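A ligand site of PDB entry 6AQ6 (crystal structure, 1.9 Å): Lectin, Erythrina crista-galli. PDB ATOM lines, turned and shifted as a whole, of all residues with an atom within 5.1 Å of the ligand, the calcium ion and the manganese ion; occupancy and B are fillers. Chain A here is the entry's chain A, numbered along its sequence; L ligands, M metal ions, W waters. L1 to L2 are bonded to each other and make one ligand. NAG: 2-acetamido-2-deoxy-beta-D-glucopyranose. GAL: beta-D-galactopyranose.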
ATOM      1  N   LEU A  86     -12.948  -7.788  -7.840  1.00  0.00           N
ATOM      2  CA  LEU A  86     -12.765  -6.713  -8.798  1.00  0.00           C
ATOM      3  C   LEU A  86     -12.034  -7.249 -10.032  1.00  0.00           C
ATOM      4  O   LEU A  86     -11.135  -8.086  -9.906  1.00  0.00           O
ATOM      5  CB  LEU A  86     -11.979  -5.571  -8.178  1.00  0.00           C
ATOM      6  CG  LEU A  86     -12.592  -4.796  -7.010  1.00  0.00           C
ATOM      7  CD1 LEU A  86     -11.658  -3.684  -6.587  1.00  0.00           C
ATOM      8  CD2 LEU A  86     -13.960  -4.233  -7.391  1.00  0.00           C
ATOM      9  N   ALA A  88      -9.563  -7.416 -13.416  1.00  0.00           N
ATOM     10  CA  ALA A  88      -8.137  -7.138 -13.591  1.00  0.00           C
ATOM     11  C   ALA A  88      -7.655  -7.812 -14.862  1.00  0.00           C
ATOM     12  O   ALA A  88      -8.273  -8.766 -15.328  1.00  0.00           O
ATOM     13  CB  ALA A  88      -7.338  -7.630 -12.380  1.00  0.00           C
ATOM     14  N   ASP A  89      -6.530  -7.344 -15.432  1.00  0.00           N
ATOM     15  CA  ASP A  89      -5.752  -6.165 -15.031  1.00  0.00           C
ATOM     16  C   ASP A  89      -5.702  -5.106 -16.148  1.00  0.00           C
ATOM     17  O   ASP A  89      -5.536  -3.925 -15.886  1.00  0.00           O
ATOM     18  CB  ASP A  89      -4.294  -6.547 -14.678  1.00  0.00           C
ATOM     19  CG  ASP A  89      -4.092  -6.853 -13.180  1.00  0.00           C
ATOM     20  OD1 ASP A  89      -4.021  -8.049 -12.857  1.00  0.00           O
ATOM     21  OD2 ASP A  89      -4.024  -5.913 -12.362  1.00  0.00           O
ATOM     22  N   TYR A 106      -0.226  -9.559 -14.332  1.00  0.00           N
ATOM     23  CA  TYR A 106      -1.012  -8.822 -13.317  1.00  0.00           C
ATOM     24  C   TYR A 106      -0.943  -7.326 -13.628  1.00  0.00           C
ATOM     25  O   TYR A 106      -1.037  -6.927 -14.808  1.00  0.00           O
ATOM     26  CB  TYR A 106      -0.523  -9.189 -11.913  1.00  0.00           C
ATOM     27  CG  TYR A 106      -0.464 -10.666 -11.627  1.00  0.00           C
ATOM     28  CD1 TYR A 106       0.543 -11.207 -10.825  1.00  0.00           C
ATOM     29  CD2 TYR A 106      -1.387 -11.538 -12.185  1.00  0.00           C
ATOM     30  CE1 TYR A 106       0.606 -12.569 -10.580  1.00  0.00           C
ATOM     31  CE2 TYR A 106      -1.328 -12.899 -11.954  1.00  0.00           C
ATOM     32  CZ  TYR A 106      -0.330 -13.412 -11.148  1.00  0.00           C
ATOM     33  OH  TYR A 106      -0.270 -14.767 -10.909  1.00  0.00           O
ATOM     34  N   GLY A 107      -0.778  -6.485 -12.615  1.00  0.00           N
ATOM     35  CA  GLY A 107      -0.749  -5.048 -12.760  1.00  0.00           C
ATOM     36  C   GLY A 107       0.440  -4.540 -13.556  1.00  0.00           C
ATOM     37  O   GLY A 107       0.483  -3.336 -13.849  1.00  0.00           O
ATOM     38  N   GLU A 127      -1.641   2.721 -21.738  1.00  0.00           N
ATOM     39  CA  GLU A 127      -2.277   1.607 -21.053  1.00  0.00           C
ATOM     40  C   GLU A 127      -3.767   1.901 -20.887  1.00  0.00           C
ATOM     41  O   GLU A 127      -4.179   3.064 -20.799  1.00  0.00           O
ATOM     42  CB  GLU A 127      -1.646   1.366 -19.682  1.00  0.00           C
ATOM     43  CG  GLU A 127      -1.915   2.482 -18.683  1.00  0.00           C
ATOM     44  CD  GLU A 127      -1.512   2.140 -17.251  1.00  0.00           C
ATOM     45  OE1 GLU A 127      -0.459   1.487 -17.047  1.00  0.00           O
ATOM     46  OE2 GLU A 127      -2.239   2.521 -16.321  1.00  0.00           O
ATOM     47  N   ASP A 129      -6.144   0.535 -18.137  1.00  0.00           N
ATOM     48  CA  ASP A 129      -5.847  -0.140 -16.877  1.00  0.00           C
ATOM     49  C   ASP A 129      -7.158  -0.337 -16.134  1.00  0.00           C
ATOM     50  O   ASP A 129      -7.873   0.643 -15.897  1.00  0.00           O
ATOM     51  CB  ASP A 129      -4.873   0.742 -16.089  1.00  0.00           C
ATOM     52  CG  ASP A 129      -4.266   0.054 -14.877  1.00  0.00           C
ATOM     53  OD1 ASP A 129      -4.875  -0.928 -14.425  1.00  0.00           O
ATOM     54  OD2 ASP A 129      -3.170   0.514 -14.383  1.00  0.00           O
ATOM     55  N   PHE A 131      -7.566  -2.286 -13.067  1.00  0.00           N
ATOM     56  CA  PHE A 131      -7.471  -2.605 -11.640  1.00  0.00           C
ATOM     57  C   PHE A 131      -6.536  -1.612 -10.962  1.00  0.00           C
ATOM     58  O   PHE A 131      -5.430  -1.368 -11.452  1.00  0.00           O
ATOM     59  CB  PHE A 131      -6.978  -4.049 -11.438  1.00  0.00           C
ATOM     60  CG  PHE A 131      -6.790  -4.431  -9.991  1.00  0.00           C
ATOM     61  CD1 PHE A 131      -7.832  -4.967  -9.265  1.00  0.00           C
ATOM     62  CD2 PHE A 131      -5.559  -4.264  -9.366  1.00  0.00           C
ATOM     63  CE1 PHE A 131      -7.678  -5.317  -7.924  1.00  0.00           C
ATOM     64  CE2 PHE A 131      -5.384  -4.620  -8.025  1.00  0.00           C
ATOM     65  CZ  PHE A 131      -6.450  -5.143  -7.306  1.00  0.00           C
ATOM     66  N   SER A 132      -6.966  -1.050  -9.837  1.00  0.00           N
ATOM     67  CA  SER A 132      -6.209   0.003  -9.152  1.00  0.00           C
ATOM     68  C   SER A 132      -5.180  -0.594  -8.189  1.00  0.00           C
ATOM     69  O   SER A 132      -5.497  -0.916  -7.039  1.00  0.00           O
ATOM     70  CB  SER A 132      -7.155   0.948  -8.420  1.00  0.00           C
ATOM     71  OG  SER A 132      -6.457   2.032  -7.819  1.00  0.00           O
ATOM     72  N   ASN A 133      -3.928  -0.709  -8.658  1.00  0.00           N
ATOM     73  CA  ASN A 133      -2.797  -1.169  -7.856  1.00  0.00           C
ATOM     74  C   ASN A 133      -2.329  -0.063  -6.914  1.00  0.00           C
ATOM     75  O   ASN A 133      -2.771   1.080  -7.024  1.00  0.00           O
ATOM     76  CB  ASN A 133      -1.634  -1.591  -8.770  1.00  0.00           C
ATOM     77  CG  ASN A 133      -1.978  -2.774  -9.658  1.00  0.00           C
ATOM     78  OD1 ASN A 133      -2.418  -2.610 -10.796  1.00  0.00           O
ATOM     79  ND2 ASN A 133      -1.733  -3.989  -9.153  1.00  0.00           N
ATOM     80  N   TRP A 135       0.268   1.690  -7.068  1.00  0.00           N
ATOM     81  CA  TRP A 135       0.899   2.771  -7.805  1.00  0.00           C
ATOM     82  C   TRP A 135      -0.059   3.523  -8.725  1.00  0.00           C
ATOM     83  O   TRP A 135       0.355   4.516  -9.329  1.00  0.00           O
ATOM     84  CB  TRP A 135       2.042   2.226  -8.665  1.00  0.00           C
ATOM     85  CG  TRP A 135       1.607   1.038  -9.510  1.00  0.00           C
ATOM     86  CD1 TRP A 135       0.936   1.073 -10.698  1.00  0.00           C
ATOM     87  CD2 TRP A 135       1.824  -0.352  -9.211  1.00  0.00           C
ATOM     88  NE1 TRP A 135       0.720  -0.199 -11.156  1.00  0.00           N
ATOM     89  CE2 TRP A 135       1.255  -1.093 -10.263  1.00  0.00           C
ATOM     90  CE3 TRP A 135       2.425  -1.026  -8.152  1.00  0.00           C
ATOM     91  CZ2 TRP A 135       1.274  -2.479 -10.294  1.00  0.00           C
ATOM     92  CZ3 TRP A 135       2.455  -2.404  -8.179  1.00  0.00           C
ATOM     93  CH2 TRP A 135       1.893  -3.124  -9.239  1.00  0.00           C
ATOM     94  N   ASP A 136      -1.323   3.036  -8.862  1.00  0.00           N
ATOM     95  CA  ASP A 136      -2.399   3.521  -9.719  1.00  0.00           C
ATOM     96  C   ASP A 136      -3.205   4.612  -9.026  1.00  0.00           C
ATOM     97  O   ASP A 136      -3.298   4.638  -7.792  1.00  0.00           O
ATOM     98  CB  ASP A 136      -3.324   2.365 -10.087  1.00  0.00           C
ATOM     99  CG  ASP A 136      -2.781   1.550 -11.213  1.00  0.00           C
ATOM    100  OD1 ASP A 136      -2.122   2.204 -12.042  1.00  0.00           O
ATOM    101  OD2 ASP A 136      -2.972   0.303 -11.261  1.00  0.00           O
ATOM    102  N   PRO A 137      -3.801   5.541  -9.779  1.00  0.00           N
ATOM    103  CA  PRO A 137      -4.821   6.406  -9.190  1.00  0.00           C
ATOM    104  C   PRO A 137      -5.981   5.552  -8.707  1.00  0.00           C
ATOM    105  O   PRO A 137      -6.045   4.364  -9.075  1.00  0.00           O
ATOM    106  CB  PRO A 137      -5.243   7.315 -10.356  1.00  0.00           C
ATOM    107  CG  PRO A 137      -4.961   6.500 -11.577  1.00  0.00           C
ATOM    108  CD  PRO A 137      -3.702   5.717 -11.236  1.00  0.00           C
ATOM    109  N   HIS A 142      -8.683   3.517 -16.408  1.00  0.00           N
ATOM    110  CA  HIS A 142      -8.061   4.785 -16.756  1.00  0.00           C
ATOM    111  C   HIS A 142      -7.084   4.548 -17.908  1.00  0.00           C
ATOM    112  O   HIS A 142      -6.484   3.475 -18.022  1.00  0.00           O
ATOM    113  CB  HIS A 142      -7.339   5.425 -15.564  1.00  0.00           C
ATOM    114  CG  HIS A 142      -6.313   4.531 -14.909  1.00  0.00           C
ATOM    115  ND1 HIS A 142      -6.508   3.973 -13.666  1.00  0.00           N
ATOM    116  CD2 HIS A 142      -5.095   4.115 -15.320  1.00  0.00           C
ATOM    117  CE1 HIS A 142      -5.458   3.244 -13.346  1.00  0.00           C
ATOM    118  NE2 HIS A 142      -4.587   3.308 -14.333  1.00  0.00           N
ATOM    119  N   ILE A 150       5.444   1.414 -15.118  1.00  0.00           N
ATOM    120  CA  ILE A 150       3.998   1.187 -15.001  1.00  0.00           C
ATOM    121  C   ILE A 150       3.322   2.306 -14.229  1.00  0.00           C
ATOM    122  O   ILE A 150       2.087   2.431 -14.270  1.00  0.00           O
ATOM    123  CB  ILE A 150       3.760  -0.186 -14.349  1.00  0.00           C
ATOM    124  CG1 ILE A 150       2.280  -0.599 -14.497  1.00  0.00           C
ATOM    125  CG2 ILE A 150       4.204  -0.139 -12.877  1.00  0.00           C
ATOM    126  CD1 ILE A 150       1.897  -1.037 -15.922  1.00  0.00           C
ATOM    127  N   SER A 152       2.232   5.687 -14.342  1.00  0.00           N
ATOM    128  CA  SER A 152       2.015   6.598 -15.455  1.00  0.00           C
ATOM    129  C   SER A 152       2.379   8.025 -15.075  1.00  0.00           C
ATOM    130  O   SER A 152       2.092   8.506 -13.970  1.00  0.00           O
ATOM    131  CB  SER A 152       0.538   6.538 -15.886  1.00  0.00           C
ATOM    132  OG  SER A 152       0.140   5.181 -15.969  1.00  0.00           O
ATOM    133  N   THR A 216      -4.833 -10.757 -17.117  1.00  0.00           N
ATOM    134  CA  THR A 216      -5.845 -10.939 -16.090  1.00  0.00           C
ATOM    135  C   THR A 216      -5.151 -11.178 -14.753  1.00  0.00           C
ATOM    136  O   THR A 216      -3.926 -11.333 -14.681  1.00  0.00           O
ATOM    137  CB  THR A 216      -6.774 -12.089 -16.434  1.00  0.00           C
ATOM    138  OG1 THR A 216      -6.010 -13.289 -16.643  1.00  0.00           O
ATOM    139  CG2 THR A 216      -7.556 -11.770 -17.710  1.00  0.00           C
ATOM    140  N   GLY A 217      -5.947 -11.236 -13.693  1.00  0.00           N
ATOM    141  CA  GLY A 217      -5.458 -10.963 -12.353  1.00  0.00           C
ATOM    142  C   GLY A 217      -4.934 -12.170 -11.595  1.00  0.00           C
ATOM    143  O   GLY A 217      -4.873 -13.292 -12.089  1.00  0.00           O
ATOM    144  N   ALA A 218      -4.570 -11.908 -10.349  1.00  0.00           N
ATOM    145  CA  ALA A 218      -3.764 -12.822  -9.528  1.00  0.00           C
ATOM    146  C   ALA A 218      -4.605 -13.663  -8.566  1.00  0.00           C
ATOM    147  O   ALA A 218      -4.041 -14.253  -7.647  1.00  0.00           O
ATOM    148  CB  ALA A 218      -2.715 -12.029  -8.745  1.00  0.00           C
ATOM    149  N   GLN A 219      -5.925 -13.730  -8.765  1.00  0.00           N
ATOM    150  CA  GLN A 219      -6.778 -14.586  -7.942  1.00  0.00           C
ATOM    151  C   GLN A 219      -7.998 -14.970  -8.757  1.00  0.00           C
ATOM    152  O   GLN A 219      -8.365 -14.276  -9.704  1.00  0.00           O
ATOM    153  CB  GLN A 219      -7.174 -13.891  -6.629  1.00  0.00           C
ATOM    154  CG  GLN A 219      -7.976 -12.611  -6.799  1.00  0.00           C
ATOM    155  CD  GLN A 219      -8.567 -12.118  -5.492  1.00  0.00           C
ATOM    156  OE1 GLN A 219      -9.657 -12.541  -5.103  1.00  0.00           O
ATOM    157  NE2 GLN A 219      -7.849 -11.221  -4.816  1.00  0.00           N
ATOM    158  N   ALA A 222     -10.738 -12.895 -10.914  1.00  0.00           N
ATOM    159  CA  ALA A 222     -10.311 -11.504 -11.099  1.00  0.00           C
ATOM    160  C   ALA A 222      -9.815 -11.377 -12.536  1.00  0.00           C
ATOM    161  O   ALA A 222      -8.613 -11.431 -12.823  1.00  0.00           O
ATOM    162  CB  ALA A 222      -9.250 -11.111 -10.091  1.00  0.00           C
HETATM  163  C1  NAG L   1      -2.540 -11.473  -2.957  1.00  0.00           C
HETATM  164  C2  NAG L   1      -3.935 -11.411  -3.544  1.00  0.00           C
HETATM  165  C3  NAG L   1      -3.780 -11.029  -5.003  1.00  0.00           C
HETATM  166  C4  NAG L   1      -3.099  -9.673  -5.084  1.00  0.00           C
HETATM  167  C5  NAG L   1      -1.898  -9.542  -4.161  1.00  0.00           C
HETATM  168  C6  NAG L   1      -1.635  -8.083  -3.897  1.00  0.00           C
HETATM  169  C7  NAG L   1      -5.738 -12.801  -2.632  1.00  0.00           C
HETATM  170  C8  NAG L   1      -6.407 -14.144  -2.510  1.00  0.00           C
HETATM  171  N2  NAG L   1      -4.556 -12.676  -3.426  1.00  0.00           N
HETATM  172  O1  NAG L   1      -2.559 -12.002  -1.651  1.00  0.00           O
HETATM  173  O3  NAG L   1      -5.039 -11.016  -5.694  1.00  0.00           O
HETATM  174  O4  NAG L   1      -2.655  -9.467  -6.412  1.00  0.00           O
HETATM  175  O5  NAG L   1      -2.086 -10.149  -2.901  1.00  0.00           O
HETATM  176  O6  NAG L   1      -0.378  -7.966  -3.260  1.00  0.00           O
HETATM  177  O7  NAG L   1      -6.232 -11.846  -2.066  1.00  0.00           O
HETATM  178  C1  GAL L   2      -3.316  -8.471  -7.128  1.00  0.00           C
HETATM  179  C2  GAL L   2      -2.519  -8.105  -8.384  1.00  0.00           C
HETATM  180  C3  GAL L   2      -3.325  -7.115  -9.195  1.00  0.00           C
HETATM  181  C4  GAL L   2      -4.628  -7.782  -9.572  1.00  0.00           C
HETATM  182  C5  GAL L   2      -5.370  -8.245  -8.322  1.00  0.00           C
HETATM  183  C6  GAL L   2      -6.597  -9.060  -8.707  1.00  0.00           C
HETATM  184  O2  GAL L   2      -1.282  -7.500  -8.055  1.00  0.00           O
HETATM  185  O3  GAL L   2      -2.583  -6.644 -10.310  1.00  0.00           O
HETATM  186  O4  GAL L   2      -4.328  -8.893 -10.372  1.00  0.00           O
HETATM  187  O5  GAL L   2      -4.572  -9.047  -7.479  1.00  0.00           O
HETATM  188  O6  GAL L   2      -7.231  -9.601  -7.554  1.00  0.00           O
HETATM  189 CA    CA M   1      -3.397  -1.344 -12.588  1.00  0.00          CA
HETATM  190 MN    MN M   2      -2.457   2.406 -14.237  1.00  0.00          MN
HETATM  191  O   HOH W   1      -0.250   1.273 -14.620  1.00  0.00           O
HETATM  192  O   HOH W   2      -1.241   4.347 -14.026  1.00  0.00           O
HETATM  193  O   HOH W   3       0.527  -6.545  -9.825  1.00  0.00           O
HETATM  194  O   HOH W   4      -1.211  -5.033  -6.428  1.00  0.00           O
HETATM  195  O   HOH W   5      -3.747  -3.425 -13.361  1.00  0.00           O
HETATM  196  O   HOH W   6      -7.050  -7.814  -4.793  1.00  0.00           O
HETATM  197  O   HOH W   7       0.801  -5.037  -4.513  1.00  0.00           O
HETATM  198  O   HOH W   8      -0.939  -1.323 -13.472  1.00  0.00           O
HETATM  199  O   HOH W   9      -9.905  -8.837  -7.661  1.00  0.00           O
HETATM  200  O   HOH W  10      -4.897  -6.910  -4.090  1.00  0.00           O
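CB of Ala 88 touches O4 of GAL L2, at 3.8 Å. CB of Tyr 106 touches O3 of GAL L2, 3.6 Å away. CA of Gly 217 touches O4 of GAL L2, at 3.1 Å. CB of Ala 222 touches O6 of GAL L2, at 3.6 Å. Hydrophobic or aromatic side chains within 4 Å of the ligand: Ala 88, Tyr 106, Phe 131, Ala 218 and Ala 222. Ten residues have an atom within 4 Å of the ligand: Ala 88, Asp 89, Tyr 106, Gly 107, Phe 131, Asn 133, Gly 217, Ala 218, Gln 219 and Ala 222.
The manganese ion is bound by OD2 of Asp 129 (2.0 Å). OE2 of Glu 127 binds the manganese ion, 2.1 Å away. The manganese ion is bound by OD1 of Asp 136 (2.2 Å). The manganese ion is bound by water W2 (2.3 Å). The manganese ion is bound by NE2 of His 142, 2.3 Å away. Water W1 binds the manganese ion.
O3 of GAL L2 is in hydrogen-bond range of ND2 of Asn 133, at 3.0 Å. The side-chain carboxylate of Asp 89 lies within hydrogen-bond range of an oxygen (O3) of GAL L2 (2.6 Å). O3 of GAL L2 is in hydrogen-bond range of N of Gly 107 (2.9 Å). The side-chain amide nitrogen of Gln 219 is in hydrogen-bond range of an oxygen (O3) of NAG L1 (3.0 Å). O4 of GAL L2 sits at hydrogen-bond distance from N of Ala 218.
The calcium ion is bound by OD2 of Asp 136 (2.2 Å). The calcium ion is bound by water W5 (2.2 Å). The calcium ion is bound by O of Phe 131 (2.3 Å). The calcium ion is bound by OD1 of Asp 129, 2.4 Å away. OD1 of Asn 133 is bound to the calcium ion (2.4 Å). The calcium ion is bound by OD2 of Asp 129. The calcium ion is bound by water W8 (2.6 Å). The calcium ion has seven donor atoms within binding distance.
Water W8 lies within hydrogen-bond range of O of Gly 107 (2.5 Å) and NE1 of Trp 135 (3.1 Å). Water W1 bridges OE1 of Glu 127 (2.4 Å) and O of Ile 150 (2.6 Å). Water W3 lies within hydrogen-bond range of O2 of GAL L2, N of Gly 107 and ND2 of Asn 133. Water W9 lies within hydrogen-bond range of O of Leu 86 (2.7 Å) and O6 of GAL L2 (2.8 Å). Water W4 bridges an oxygen (O2) of GAL L2 (3.0 Å) and the side-chain amide nitrogen of Asn 133 (3.0 Å). Water W6 lies within hydrogen-bond range of an oxygen (O6) of GAL L2 and the side-chain amide nitrogen of Gln 219.
Four residues have an atom within 4 Å of the calcium ion: Asp 129, Phe 131, Asn 133 and Asp 136.
The side-chain carboxylate (OD2) of Asp 89 sits at hydrogen-bond distance from the backbone NH (N) of Gly 107. O of Ala 222 is in hydrogen-bond range of N of Gly 217 (2.8 Å).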
